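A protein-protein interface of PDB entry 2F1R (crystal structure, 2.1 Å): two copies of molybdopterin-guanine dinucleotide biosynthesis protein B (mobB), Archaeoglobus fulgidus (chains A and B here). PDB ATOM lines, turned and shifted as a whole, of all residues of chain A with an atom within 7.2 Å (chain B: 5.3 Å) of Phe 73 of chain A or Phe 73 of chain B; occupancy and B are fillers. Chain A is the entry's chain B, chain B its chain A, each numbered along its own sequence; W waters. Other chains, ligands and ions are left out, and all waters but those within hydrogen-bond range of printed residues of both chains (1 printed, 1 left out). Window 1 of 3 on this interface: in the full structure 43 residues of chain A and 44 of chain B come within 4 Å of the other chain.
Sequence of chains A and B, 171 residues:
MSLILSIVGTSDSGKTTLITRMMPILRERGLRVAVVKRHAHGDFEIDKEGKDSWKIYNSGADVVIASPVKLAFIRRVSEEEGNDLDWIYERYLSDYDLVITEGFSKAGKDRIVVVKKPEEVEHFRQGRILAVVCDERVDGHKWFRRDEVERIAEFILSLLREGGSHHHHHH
The backbone NH of Asp 62 of chain B sits at hydrogen-bond distance from the backbone carbonyl oxygen of Val 33 of chain A, 3.1 Å away.
N of Val 35 of chain A lies within hydrogen-bond range of O of Asp 62 of chain B (2.8 Å).
The side-chain carboxylate (OD2) of Asp 62 of chain B lies within hydrogen-bond range of the side-chain hydroxyl (OH) of Tyr 96 of chain A (2.6 Å).
N of Val 64 of chain B lies within hydrogen-bond range of O of Val 35 of chain A, at 2.8 Å.
The backbone NH (N) of Arg 75 of chain A lies within hydrogen-bond range of the backbone carbonyl oxygen (O) of Leu 71 of chain B (2.9 Å).
N of Phe 73 of chain B is in hydrogen-bond range of O of Phe 73 of chain A (2.8 Å).
N of Leu 71 of chain A lies within hydrogen-bond range of O of Arg 75 of chain B (2.8 Å).
The guanidinium group of Arg 75 of chain B is in salt-bridge range of the side-chain carboxylate of Asp 95 of chain A (3.9 Å).
The side-chain hydroxyl (OH) of Tyr 96 of chain A lies within hydrogen-bond range of the guanidinium group (NH1) of Arg 75 of chain B (3.5 Å).
OH of Tyr 96 of chain B sits at hydrogen-bond distance from OD2 of Asp 62 of chain A, at 2.5 Å.
O of Leu 71 of chain A lies close to O of Phe 73 of chain B (3.4 Å).
The backbone carbonyl oxygen of Val 63 of chain B sits at hydrogen-bond distance from the backbone NH of Ile 74 of chain B (2.9 Å).
The backbone carbonyl oxygen (O) of Ala 72 of chain B lies within hydrogen-bond range of the backbone NH (N) of Ile 65 of chain B, at 2.8 Å.
The side-chain carboxylate (OD1) of Asp 62 of chain A lies within salt-bridge range of the guanidinium group (NH1) of Arg 76 of chain A, at 3.6 Å.
The backbone NH of Ile 74 of chain A is in hydrogen-bond range of the backbone carbonyl oxygen of Val 63 of chain A.
O of Ala 72 of chain A is in hydrogen-bond range of N of Ile 65 of chain A (2.7 Å).
NH1 of Arg 75 of chain A sits at hydrogen-bond distance from OH of Tyr 92 of chain A, at 2.8 Å.
Val 63 of chain B touches Val 35 of chain A.
Val 64 of chain A touches Leu 93 of chain B (CG2 to CD2, 3.8 Å).
Tyr 92 of chain B touches Leu 71 of chain A (CE2 to CD2, 3.3 Å).
O of Phe 73 of chain A touches O of Leu 71 of chain B, 3.6 Å away.
Phe 73 of chain A touches Ala 72 of chain B.
Phe 73 of chain A touches Leu 93 of chain B (CE1 to CD2, 3.998 Å).
Phe 73 of chain A touches Tyr 96 of chain B.
Ile 74 of chain A touches Leu 71 of chain B (CA to O, 3.3 Å).
Tyr 92 of chain A touches Phe 73 of chain B.
Tyr 96 of chain A touches Phe 73 of chain B.
Of the printed residues of chain B, Phe 73 of chain A touches Leu 71 (3.6 Å), Ala 72 (3.2 Å), Phe 73 (2.8 Å), Tyr 92 (3.3 Å), Leu 93 (3.998 Å) and Tyr 96 (3.5 Å).
Phe 73 of chain B touches six residues of chain A.
Of the printed residues of chain A, Val 63 of chain B touches Val 35.
Printed residues of chain A within 4 Å of Tyr 96 of chain B: Asp 62, Phe 73 and Arg 75.
Of the printed residues of chain A, Asp 62 of chain B touches Val 33 (3.1 Å), Ala 34 (3.2 Å), Val 35 (2.8 Å) and Tyr 96 (2.6 Å).
Of the printed residues of chain B, Tyr 92 of chain A touches Phe 73 (3.9 Å).
Arg 76 of chain A touches none of the printed residues of chain B.
The nearest printed residue of chain B that does not touch Phe 73 of chain A is Ile 74 of chain B (5.1 Å).
Of the 12 printed residues of chain B, 11 touch a printed residue of chain A.
Printed residues of chain B that touch a printed residue of chain A: Asp 62, Val 63, Val 64, Leu 71, Ala 72, Phe 73, Ile 74, Arg 75, Tyr 92, Leu 93 and Tyr 96.
Of the 18 printed residues of chain A, 14 touch a printed residue of chain B.
Among the printed residues, 28 pairs touch across the chains.
Asp 62 of chain A touches Tyr 96 of chain B, and with the chains exchanged Tyr 96 of chain A touches Asp 62 of chain B.
Val 64 of chain A touches Leu 93 of chain B, and with the chains exchanged Leu 93 of chain A touches Val 64 of chain B.
Ala 72 of chain A touches Phe 73 of chain B, and with the chains exchanged Phe 73 of chain A touches Ala 72 of chain B.
Phe 73 of chain A touches Tyr 92 of chain B, and with the chains exchanged Tyr 92 of chain A touches Phe 73 of chain B.
Of the 28 pairs that touch across the chains among the printed residues, 21 have their exchanged pair printed and touching as well.
Water W1 lies within hydrogen-bond range of the side-chain hydroxyl (OH) of Tyr 92 of chain A (2.5 Å), the backbone carbonyl oxygen (O) of Tyr 92 of chain B (2.7 Å) and the guanidinium group (NH2) of Arg 91 of chain A (3.1 Å).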
ATOM      1  N   VAL A  33     -19.282 -26.612  -9.183  1.00  0.00           N
ATOM      2  CA  VAL A  33     -19.427 -25.275  -8.602  1.00  0.00           C
ATOM      3  C   VAL A  33     -18.114 -24.545  -8.646  1.00  0.00           C
ATOM      4  O   VAL A  33     -17.084 -25.110  -8.338  1.00  0.00           O
ATOM      5  CB  VAL A  33     -19.929 -25.358  -7.131  1.00  0.00           C
ATOM      6  CG1 VAL A  33     -20.224 -23.939  -6.528  1.00  0.00           C
ATOM      7  CG2 VAL A  33     -21.161 -26.249  -7.037  1.00  0.00           C
ATOM      8  N   ALA A  34     -18.152 -23.286  -9.041  1.00  0.00           N
ATOM      9  CA  ALA A  34     -17.004 -22.396  -8.912  1.00  0.00           C
ATOM     10  C   ALA A  34     -17.376 -21.221  -7.996  1.00  0.00           C
ATOM     11  O   ALA A  34     -18.556 -20.839  -7.930  1.00  0.00           O
ATOM     12  CB  ALA A  34     -16.622 -21.884 -10.262  1.00  0.00           C
ATOM     13  N   VAL A  35     -16.399 -20.692  -7.273  1.00  0.00           N
ATOM     14  CA  VAL A  35     -16.563 -19.501  -6.461  1.00  0.00           C
ATOM     15  C   VAL A  35     -15.590 -18.445  -6.928  1.00  0.00           C
ATOM     16  O   VAL A  35     -14.389 -18.708  -7.011  1.00  0.00           O
ATOM     17  CB  VAL A  35     -16.308 -19.788  -4.960  1.00  0.00           C
ATOM     18  CG1 VAL A  35     -16.284 -18.496  -4.130  1.00  0.00           C
ATOM     19  CG2 VAL A  35     -17.369 -20.786  -4.391  1.00  0.00           C
ATOM     20  N   ASP A  62       1.967 -14.907 -18.487  1.00  0.00           N
ATOM     21  CA  ASP A  62       0.897 -15.563 -17.683  1.00  0.00           C
ATOM     22  C   ASP A  62       1.374 -17.007 -17.428  1.00  0.00           C
ATOM     23  O   ASP A  62       2.230 -17.512 -18.183  1.00  0.00           O
ATOM     24  CB  ASP A  62      -0.461 -15.526 -18.398  1.00  0.00           C
ATOM     25  CG  ASP A  62      -0.934 -14.117 -18.668  1.00  0.00           C
ATOM     26  OD1 ASP A  62      -0.462 -13.232 -17.998  1.00  0.00           O
ATOM     27  OD2 ASP A  62      -1.758 -13.858 -19.572  1.00  0.00           O
ATOM     28  N   VAL A  63       0.883 -17.642 -16.356  1.00  0.00           N
ATOM     29  CA  VAL A  63       1.418 -18.940 -15.930  1.00  0.00           C
ATOM     30  C   VAL A  63       0.296 -19.918 -15.723  1.00  0.00           C
ATOM     31  O   VAL A  63      -0.693 -19.601 -15.058  1.00  0.00           O
ATOM     32  CB  VAL A  63       2.185 -18.864 -14.541  1.00  0.00           C
ATOM     33  CG1 VAL A  63       2.984 -20.129 -14.295  1.00  0.00           C
ATOM     34  CG2 VAL A  63       3.162 -17.720 -14.531  1.00  0.00           C
ATOM     35  N   VAL A  64       0.476 -21.128 -16.255  1.00  0.00           N
ATOM     36  CA  VAL A  64      -0.208 -22.325 -15.758  1.00  0.00           C
ATOM     37  C   VAL A  64       0.768 -23.183 -14.889  1.00  0.00           C
ATOM     38  O   VAL A  64       1.869 -23.549 -15.334  1.00  0.00           O
ATOM     39  CB  VAL A  64      -0.794 -23.223 -16.899  1.00  0.00           C
ATOM     40  CG1 VAL A  64      -1.473 -24.495 -16.309  1.00  0.00           C
ATOM     41  CG2 VAL A  64      -1.794 -22.439 -17.792  1.00  0.00           C
ATOM     42  N   ILE A  65       0.327 -23.510 -13.672  1.00  0.00           N
ATOM     43  CA  ILE A  65       0.991 -24.514 -12.822  1.00  0.00           C
ATOM     44  C   ILE A  65       0.151 -25.772 -12.763  1.00  0.00           C
ATOM     45  O   ILE A  65      -0.944 -25.754 -12.223  1.00  0.00           O
ATOM     46  CB  ILE A  65       1.233 -23.976 -11.430  1.00  0.00           C
ATOM     47  CG1 ILE A  65       2.070 -22.688 -11.538  1.00  0.00           C
ATOM     48  CG2 ILE A  65       1.977 -25.029 -10.571  1.00  0.00           C
ATOM     49  CD1 ILE A  65       1.471 -21.532 -10.772  1.00  0.00           C
ATOM     50  N   LEU A  71      -5.018 -27.714 -11.103  1.00  0.00           N
ATOM     51  CA  LEU A  71      -4.408 -26.791 -12.064  1.00  0.00           C
ATOM     52  C   LEU A  71      -4.613 -25.340 -11.635  1.00  0.00           C
ATOM     53  O   LEU A  71      -5.678 -24.904 -11.229  1.00  0.00           O
ATOM     54  CB  LEU A  71      -5.000 -27.023 -13.458  1.00  0.00           C
ATOM     55  CG  LEU A  71      -4.438 -26.161 -14.589  1.00  0.00           C
ATOM     56  CD1 LEU A  71      -3.984 -27.032 -15.750  1.00  0.00           C
ATOM     57  CD2 LEU A  71      -5.470 -25.145 -15.054  1.00  0.00           C
ATOM     58  N   ALA A  72      -3.537 -24.515 -11.736  1.00  0.00           N
ATOM     59  CA  ALA A  72      -3.645 -23.080 -11.459  1.00  0.00           C
ATOM     60  C   ALA A  72      -3.212 -22.238 -12.656  1.00  0.00           C
ATOM     61  O   ALA A  72      -2.206 -22.523 -13.279  1.00  0.00           O
ATOM     62  CB  ALA A  72      -2.861 -22.711 -10.201  1.00  0.00           C
ATOM     63  N   PHE A  73      -4.000 -21.221 -12.969  1.00  0.00           N
ATOM     64  CA  PHE A  73      -3.776 -20.364 -14.115  1.00  0.00           C
ATOM     65  C   PHE A  73      -3.835 -18.949 -13.576  1.00  0.00           C
ATOM     66  O   PHE A  73      -4.849 -18.547 -12.994  1.00  0.00           O
ATOM     67  CB  PHE A  73      -4.835 -20.627 -15.186  1.00  0.00           C
ATOM     68  CG  PHE A  73      -4.780 -19.660 -16.399  1.00  0.00           C
ATOM     69  CD1 PHE A  73      -3.567 -19.386 -17.086  1.00  0.00           C
ATOM     70  CD2 PHE A  73      -5.937 -19.071 -16.873  1.00  0.00           C
ATOM     71  CE1 PHE A  73      -3.541 -18.543 -18.193  1.00  0.00           C
ATOM     72  CE2 PHE A  73      -5.919 -18.227 -17.995  1.00  0.00           C
ATOM     73  CZ  PHE A  73      -4.709 -17.979 -18.653  1.00  0.00           C
ATOM     74  N   ILE A  74      -2.727 -18.228 -13.705  1.00  0.00           N
ATOM     75  CA  ILE A  74      -2.658 -16.848 -13.322  1.00  0.00           C
ATOM     76  C   ILE A  74      -2.385 -15.986 -14.523  1.00  0.00           C
ATOM     77  O   ILE A  74      -1.365 -16.159 -15.174  1.00  0.00           O
ATOM     78  CB  ILE A  74      -1.516 -16.578 -12.280  1.00  0.00           C
ATOM     79  CG1 ILE A  74      -1.586 -17.579 -11.095  1.00  0.00           C
ATOM     80  CG2 ILE A  74      -1.642 -15.137 -11.777  1.00  0.00           C
ATOM     81  CD1 ILE A  74      -0.656 -18.767 -11.199  1.00  0.00           C
ATOM     82  N   ARG A  75      -3.276 -15.039 -14.793  1.00  0.00           N
ATOM     83  CA  ARG A  75      -3.120 -14.161 -15.935  1.00  0.00           C
ATOM     84  C   ARG A  75      -3.373 -12.666 -15.657  1.00  0.00           C
ATOM     85  O   ARG A  75      -4.246 -12.322 -14.870  1.00  0.00           O
ATOM     86  CB  ARG A  75      -4.024 -14.638 -17.063  1.00  0.00           C
ATOM     87  CG  ARG A  75      -5.517 -14.631 -16.770  1.00  0.00           C
ATOM     88  CD  ARG A  75      -6.352 -14.603 -18.112  1.00  0.00           C
ATOM     89  NE  ARG A  75      -6.186 -13.332 -18.795  1.00  0.00           N
ATOM     90  CZ  ARG A  75      -6.776 -12.988 -19.941  1.00  0.00           C
ATOM     91  NH1 ARG A  75      -7.604 -13.818 -20.562  1.00  0.00           N
ATOM     92  NH2 ARG A  75      -6.560 -11.786 -20.444  1.00  0.00           N
ATOM     93  N   ARG A  76      -2.638 -11.803 -16.369  1.00  0.00           N
ATOM     94  CA  ARG A  76      -2.921 -10.388 -16.431  1.00  0.00           C
ATOM     95  C   ARG A  76      -4.257 -10.178 -17.120  1.00  0.00           C
ATOM     96  O   ARG A  76      -4.613 -10.875 -18.115  1.00  0.00           O
ATOM     97  CB  ARG A  76      -1.824  -9.667 -17.224  1.00  0.00           C
ATOM     98  CG  ARG A  76      -0.443  -9.871 -16.649  1.00  0.00           C
ATOM     99  CD  ARG A  76       0.712  -9.581 -17.646  1.00  0.00           C
ATOM    100  NE  ARG A  76       1.866  -9.321 -16.790  1.00  0.00           N
ATOM    101  CZ  ARG A  76       2.590 -10.288 -16.246  1.00  0.00           C
ATOM    102  NH1 ARG A  76       2.304 -11.550 -16.541  1.00  0.00           N
ATOM    103  NH2 ARG A  76       3.593  -9.983 -15.417  1.00  0.00           N
ATOM    104  N   ARG A  91     -15.833 -16.756 -20.401  1.00  0.00           N
ATOM    105  CA  ARG A  91     -14.516 -17.217 -20.806  1.00  0.00           C
ATOM    106  C   ARG A  91     -14.184 -18.547 -20.152  1.00  0.00           C
ATOM    107  O   ARG A  91     -13.862 -19.520 -20.876  1.00  0.00           O
ATOM    108  CB  ARG A  91     -13.449 -16.176 -20.471  1.00  0.00           C
ATOM    109  CG  ARG A  91     -12.045 -16.571 -20.904  1.00  0.00           C
ATOM    110  CD  ARG A  91     -11.942 -16.662 -22.418  1.00  0.00           C
ATOM    111  NE  ARG A  91     -10.784 -17.445 -22.842  1.00  0.00           N
ATOM    112  CZ  ARG A  91     -10.715 -18.770 -22.774  1.00  0.00           C
ATOM    113  NH1 ARG A  91     -11.741 -19.463 -22.299  1.00  0.00           N
ATOM    114  NH2 ARG A  91      -9.622 -19.399 -23.183  1.00  0.00           N
ATOM    115  N   TYR A  92     -14.294 -18.665 -18.818  1.00  0.00           N
ATOM    116  CA  TYR A  92     -13.706 -19.774 -18.046  1.00  0.00           C
ATOM    117  C   TYR A  92     -14.646 -20.691 -17.275  1.00  0.00           C
ATOM    118  O   TYR A  92     -14.225 -21.779 -16.873  1.00  0.00           O
ATOM    119  CB  TYR A  92     -12.645 -19.240 -17.057  1.00  0.00           C
ATOM    120  CG  TYR A  92     -11.541 -18.447 -17.729  1.00  0.00           C
ATOM    121  CD1 TYR A  92     -10.569 -19.102 -18.510  1.00  0.00           C
ATOM    122  CD2 TYR A  92     -11.465 -17.045 -17.598  1.00  0.00           C
ATOM    123  CE1 TYR A  92      -9.572 -18.382 -19.156  1.00  0.00           C
ATOM    124  CE2 TYR A  92     -10.457 -16.324 -18.235  1.00  0.00           C
ATOM    125  CZ  TYR A  92      -9.499 -17.012 -19.011  1.00  0.00           C
ATOM    126  OH  TYR A  92      -8.478 -16.345 -19.679  1.00  0.00           O
ATOM    127  N   LEU A  93     -15.899 -20.295 -17.077  1.00  0.00           N
ATOM    128  CA  LEU A  93     -16.760 -20.992 -16.145  1.00  0.00           C
ATOM    129  C   LEU A  93     -18.062 -21.492 -16.743  1.00  0.00           C
ATOM    130  O   LEU A  93     -18.991 -21.837 -16.004  1.00  0.00           O
ATOM    131  CB  LEU A  93     -17.098 -20.065 -14.976  1.00  0.00           C
ATOM    132  CG  LEU A  93     -15.896 -19.434 -14.253  1.00  0.00           C
ATOM    133  CD1 LEU A  93     -16.429 -18.520 -13.226  1.00  0.00           C
ATOM    134  CD2 LEU A  93     -14.965 -20.492 -13.657  1.00  0.00           C
ATOM    135  N   ASP A  95     -18.981 -24.139 -18.235  1.00  0.00           N
ATOM    136  CA  ASP A  95     -19.247 -25.544 -17.933  1.00  0.00           C
ATOM    137  C   ASP A  95     -19.790 -25.807 -16.516  1.00  0.00           C
ATOM    138  O   ASP A  95     -20.201 -26.928 -16.205  1.00  0.00           O
ATOM    139  CB  ASP A  95     -17.958 -26.359 -18.143  1.00  0.00           C
ATOM    140  CG  ASP A  95     -16.687 -25.669 -17.545  1.00  0.00           C
ATOM    141  OD1 ASP A  95     -16.563 -24.368 -17.525  1.00  0.00           O
ATOM    142  OD2 ASP A  95     -15.785 -26.466 -17.111  1.00  0.00           O
ATOM    143  N   TYR A  96     -19.764 -24.800 -15.651  1.00  0.00           N
ATOM    144  CA  TYR A  96     -20.258 -24.936 -14.282  1.00  0.00           C
ATOM    145  C   TYR A  96     -21.762 -24.840 -14.140  1.00  0.00           C
ATOM    146  O   TYR A  96     -22.408 -24.070 -14.831  1.00  0.00           O
ATOM    147  CB  TYR A  96     -19.574 -23.933 -13.355  1.00  0.00           C
ATOM    148  CG  TYR A  96     -18.117 -24.295 -13.183  1.00  0.00           C
ATOM    149  CD1 TYR A  96     -17.695 -25.106 -12.119  1.00  0.00           C
ATOM    150  CD2 TYR A  96     -17.185 -23.867 -14.095  1.00  0.00           C
ATOM    151  CE1 TYR A  96     -16.356 -25.464 -11.959  1.00  0.00           C
ATOM    152  CE2 TYR A  96     -15.852 -24.225 -13.974  1.00  0.00           C
ATOM    153  CZ  TYR A  96     -15.446 -25.010 -12.898  1.00  0.00           C
ATOM    154  OH  TYR A  96     -14.119 -25.334 -12.787  1.00  0.00           O
ATOM    155  N   ASP B  62     -14.174 -25.127  -7.223  1.00  0.00           N
ATOM    156  CA  ASP B  62     -13.089 -24.491  -7.974  1.00  0.00           C
ATOM    157  C   ASP B  62     -13.154 -22.992  -7.700  1.00  0.00           C
ATOM    158  O   ASP B  62     -14.224 -22.458  -7.368  1.00  0.00           O
ATOM    159  CB  ASP B  62     -13.232 -24.816  -9.447  1.00  0.00           C
ATOM    160  CG  ASP B  62     -12.988 -26.313  -9.721  1.00  0.00           C
ATOM    161  OD1 ASP B  62     -12.244 -26.977  -8.905  1.00  0.00           O
ATOM    162  OD2 ASP B  62     -13.491 -26.804 -10.772  1.00  0.00           O
ATOM    163  N   VAL B  63     -12.002 -22.318  -7.761  1.00  0.00           N
ATOM    164  CA  VAL B  63     -11.915 -20.968  -7.235  1.00  0.00           C
ATOM    165  C   VAL B  63     -11.343 -19.965  -8.271  1.00  0.00           C
ATOM    166  O   VAL B  63     -10.349 -20.259  -8.933  1.00  0.00           O
ATOM    167  CB  VAL B  63     -11.035 -20.972  -5.960  1.00  0.00           C
ATOM    168  CG1 VAL B  63     -10.809 -19.543  -5.427  1.00  0.00           C
ATOM    169  CG2 VAL B  63     -11.724 -21.826  -4.859  1.00  0.00           C
ATOM    170  N   VAL B  64     -12.010 -18.823  -8.425  1.00  0.00           N
ATOM    171  CA  VAL B  64     -11.444 -17.694  -9.200  1.00  0.00           C
ATOM    172  C   VAL B  64     -11.170 -16.548  -8.251  1.00  0.00           C
ATOM    173  O   VAL B  64     -12.068 -16.117  -7.532  1.00  0.00           O
ATOM    174  CB  VAL B  64     -12.350 -17.210 -10.382  1.00  0.00           C
ATOM    175  CG1 VAL B  64     -11.774 -15.977 -11.047  1.00  0.00           C
ATOM    176  CG2 VAL B  64     -12.504 -18.260 -11.442  1.00  0.00           C
ATOM    177  N   ILE B  65      -9.926 -16.094  -8.213  1.00  0.00           N
ATOM    178  CA  ILE B  65      -9.567 -14.914  -7.449  1.00  0.00           C
ATOM    179  C   ILE B  65      -9.389 -13.791  -8.441  1.00  0.00           C
ATOM    180  O   ILE B  65      -8.516 -13.848  -9.308  1.00  0.00           O
ATOM    181  CB  ILE B  65      -8.303 -15.127  -6.612  1.00  0.00           C
ATOM    182  CG1 ILE B  65      -8.451 -16.409  -5.809  1.00  0.00           C
ATOM    183  CG2 ILE B  65      -8.135 -14.001  -5.600  1.00  0.00           C
ATOM    184  CD1 ILE B  65      -7.247 -16.758  -4.921  1.00  0.00           C
ATOM    185  N   LEU B  71      -5.943 -12.266 -12.451  1.00  0.00           N
ATOM    186  CA  LEU B  71      -6.922 -13.314 -12.152  1.00  0.00           C
ATOM    187  C   LEU B  71      -6.240 -14.670 -11.985  1.00  0.00           C
ATOM    188  O   LEU B  71      -5.300 -14.987 -12.760  1.00  0.00           O
ATOM    189  CB  LEU B  71      -7.973 -13.380 -13.265  1.00  0.00           C
ATOM    190  CG  LEU B  71      -9.248 -14.166 -12.954  1.00  0.00           C
ATOM    191  CD1 LEU B  71     -10.465 -13.461 -13.532  1.00  0.00           C
ATOM    192  CD2 LEU B  71      -9.147 -15.586 -13.490  1.00  0.00           C
ATOM    193  N   ALA B  72      -6.628 -15.428 -10.987  1.00  0.00           N
ATOM    194  CA  ALA B  72      -6.087 -16.760 -10.711  1.00  0.00           C
ATOM    195  C   ALA B  72      -7.270 -17.686 -10.733  1.00  0.00           C
ATOM    196  O   ALA B  72      -8.285 -17.378 -10.103  1.00  0.00           O
ATOM    197  CB  ALA B  72      -5.384 -16.804  -9.340  1.00  0.00           C
ATOM    198  N   PHE B  73      -7.173 -18.749 -11.522  1.00  0.00           N
ATOM    199  CA  PHE B  73      -8.173 -19.841 -11.585  1.00  0.00           C
ATOM    200  C   PHE B  73      -7.498 -21.114 -11.047  1.00  0.00           C
ATOM    201  O   PHE B  73      -6.468 -21.566 -11.570  1.00  0.00           O
ATOM    202  CB  PHE B  73      -8.714 -20.015 -13.033  1.00  0.00           C
ATOM    203  CG  PHE B  73      -9.881 -21.032 -13.181  1.00  0.00           C
ATOM    204  CD1 PHE B  73     -10.794 -21.298 -12.128  1.00  0.00           C
ATOM    205  CD2 PHE B  73     -10.107 -21.671 -14.418  1.00  0.00           C
ATOM    206  CE1 PHE B  73     -11.874 -22.218 -12.294  1.00  0.00           C
ATOM    207  CE2 PHE B  73     -11.200 -22.565 -14.610  1.00  0.00           C
ATOM    208  CZ  PHE B  73     -12.078 -22.843 -13.522  1.00  0.00           C
ATOM    209  N   ILE B  74      -8.064 -21.657  -9.981  1.00  0.00           N
ATOM    210  CA  ILE B  74      -7.562 -22.852  -9.337  1.00  0.00           C
ATOM    211  C   ILE B  74      -8.652 -23.917  -9.426  1.00  0.00           C
ATOM    212  O   ILE B  74      -9.775 -23.676  -9.005  1.00  0.00           O
ATOM    213  CB  ILE B  74      -7.218 -22.564  -7.881  1.00  0.00           C
ATOM    214  CG1 ILE B  74      -6.380 -21.257  -7.805  1.00  0.00           C
ATOM    215  CG2 ILE B  74      -6.502 -23.801  -7.247  1.00  0.00           C
ATOM    216  CD1 ILE B  74      -6.210 -20.643  -6.404  1.00  0.00           C
ATOM    217  N   ARG B  75      -8.331 -25.060 -10.025  1.00  0.00           N
ATOM    218  CA  ARG B  75      -9.333 -26.073 -10.266  1.00  0.00           C
ATOM    219  C   ARG B  75      -8.875 -27.537 -10.238  1.00  0.00           C
ATOM    220  O   ARG B  75      -7.787 -27.862 -10.682  1.00  0.00           O
ATOM    221  CB  ARG B  75     -10.055 -25.780 -11.577  1.00  0.00           C
ATOM    222  CG  ARG B  75      -9.190 -25.856 -12.764  1.00  0.00           C
ATOM    223  CD  ARG B  75     -10.083 -25.951 -13.956  1.00  0.00           C
ATOM    224  NE  ARG B  75     -10.397 -27.296 -14.329  1.00  0.00           N
ATOM    225  CZ  ARG B  75     -11.459 -27.631 -15.048  1.00  0.00           C
ATOM    226  NH1 ARG B  75     -12.330 -26.698 -15.416  1.00  0.00           N
ATOM    227  NH2 ARG B  75     -11.674 -28.918 -15.363  1.00  0.00           N
ATOM    228  N   TYR B  92      -7.349 -23.018 -21.906  1.00  0.00           N
ATOM    229  CA  TYR B  92      -6.747 -21.870 -21.264  1.00  0.00           C
ATOM    230  C   TYR B  92      -5.944 -20.951 -22.167  1.00  0.00           C
ATOM    231  O   TYR B  92      -5.816 -19.773 -21.880  1.00  0.00           O
ATOM    232  CB  TYR B  92      -5.838 -22.345 -20.135  1.00  0.00           C
ATOM    233  CG  TYR B  92      -6.591 -22.815 -18.928  1.00  0.00           C
ATOM    234  CD1 TYR B  92      -7.091 -21.905 -18.007  1.00  0.00           C
ATOM    235  CD2 TYR B  92      -6.817 -24.164 -18.713  1.00  0.00           C
ATOM    236  CE1 TYR B  92      -7.788 -22.321 -16.901  1.00  0.00           C
ATOM    237  CE2 TYR B  92      -7.522 -24.600 -17.603  1.00  0.00           C
ATOM    238  CZ  TYR B  92      -7.995 -23.661 -16.698  1.00  0.00           C
ATOM    239  OH  TYR B  92      -8.703 -24.082 -15.588  1.00  0.00           O
ATOM    240  N   LEU B  93      -5.377 -21.507 -23.224  1.00  0.00           N
ATOM    241  CA  LEU B  93      -4.227 -20.887 -23.838  1.00  0.00           C
ATOM    242  C   LEU B  93      -4.409 -20.562 -25.315  1.00  0.00           C
ATOM    243  O   LEU B  93      -3.463 -20.146 -25.975  1.00  0.00           O
ATOM    244  CB  LEU B  93      -2.986 -21.785 -23.617  1.00  0.00           C
ATOM    245  CG  LEU B  93      -2.505 -22.092 -22.175  1.00  0.00           C
ATOM    246  CD1 LEU B  93      -1.116 -22.685 -22.174  1.00  0.00           C
ATOM    247  CD2 LEU B  93      -2.514 -20.913 -21.245  1.00  0.00           C
ATOM    248  N   TYR B  96      -3.108 -17.084 -26.916  1.00  0.00           N
ATOM    249  CA  TYR B  96      -1.741 -16.646 -26.805  1.00  0.00           C
ATOM    250  C   TYR B  96      -1.018 -16.740 -28.126  1.00  0.00           C
ATOM    251  O   TYR B  96      -1.328 -17.569 -28.964  1.00  0.00           O
ATOM    252  CB  TYR B  96      -1.030 -17.487 -25.749  1.00  0.00           C
ATOM    253  CG  TYR B  96      -1.503 -17.042 -24.417  1.00  0.00           C
ATOM    254  CD1 TYR B  96      -0.863 -16.024 -23.750  1.00  0.00           C
ATOM    255  CD2 TYR B  96      -2.641 -17.629 -23.819  1.00  0.00           C
ATOM    256  CE1 TYR B  96      -1.311 -15.605 -22.493  1.00  0.00           C
ATOM    257  CE2 TYR B  96      -3.096 -17.220 -22.564  1.00  0.00           C
ATOM    258  CZ  TYR B  96      -2.440 -16.202 -21.903  1.00  0.00           C
ATOM    259  OH  TYR B  96      -2.902 -15.788 -20.622  1.00  0.00           O
HETATM  260  O   HOH W   1      -7.535 -17.713 -21.598  1.00  0.00           O
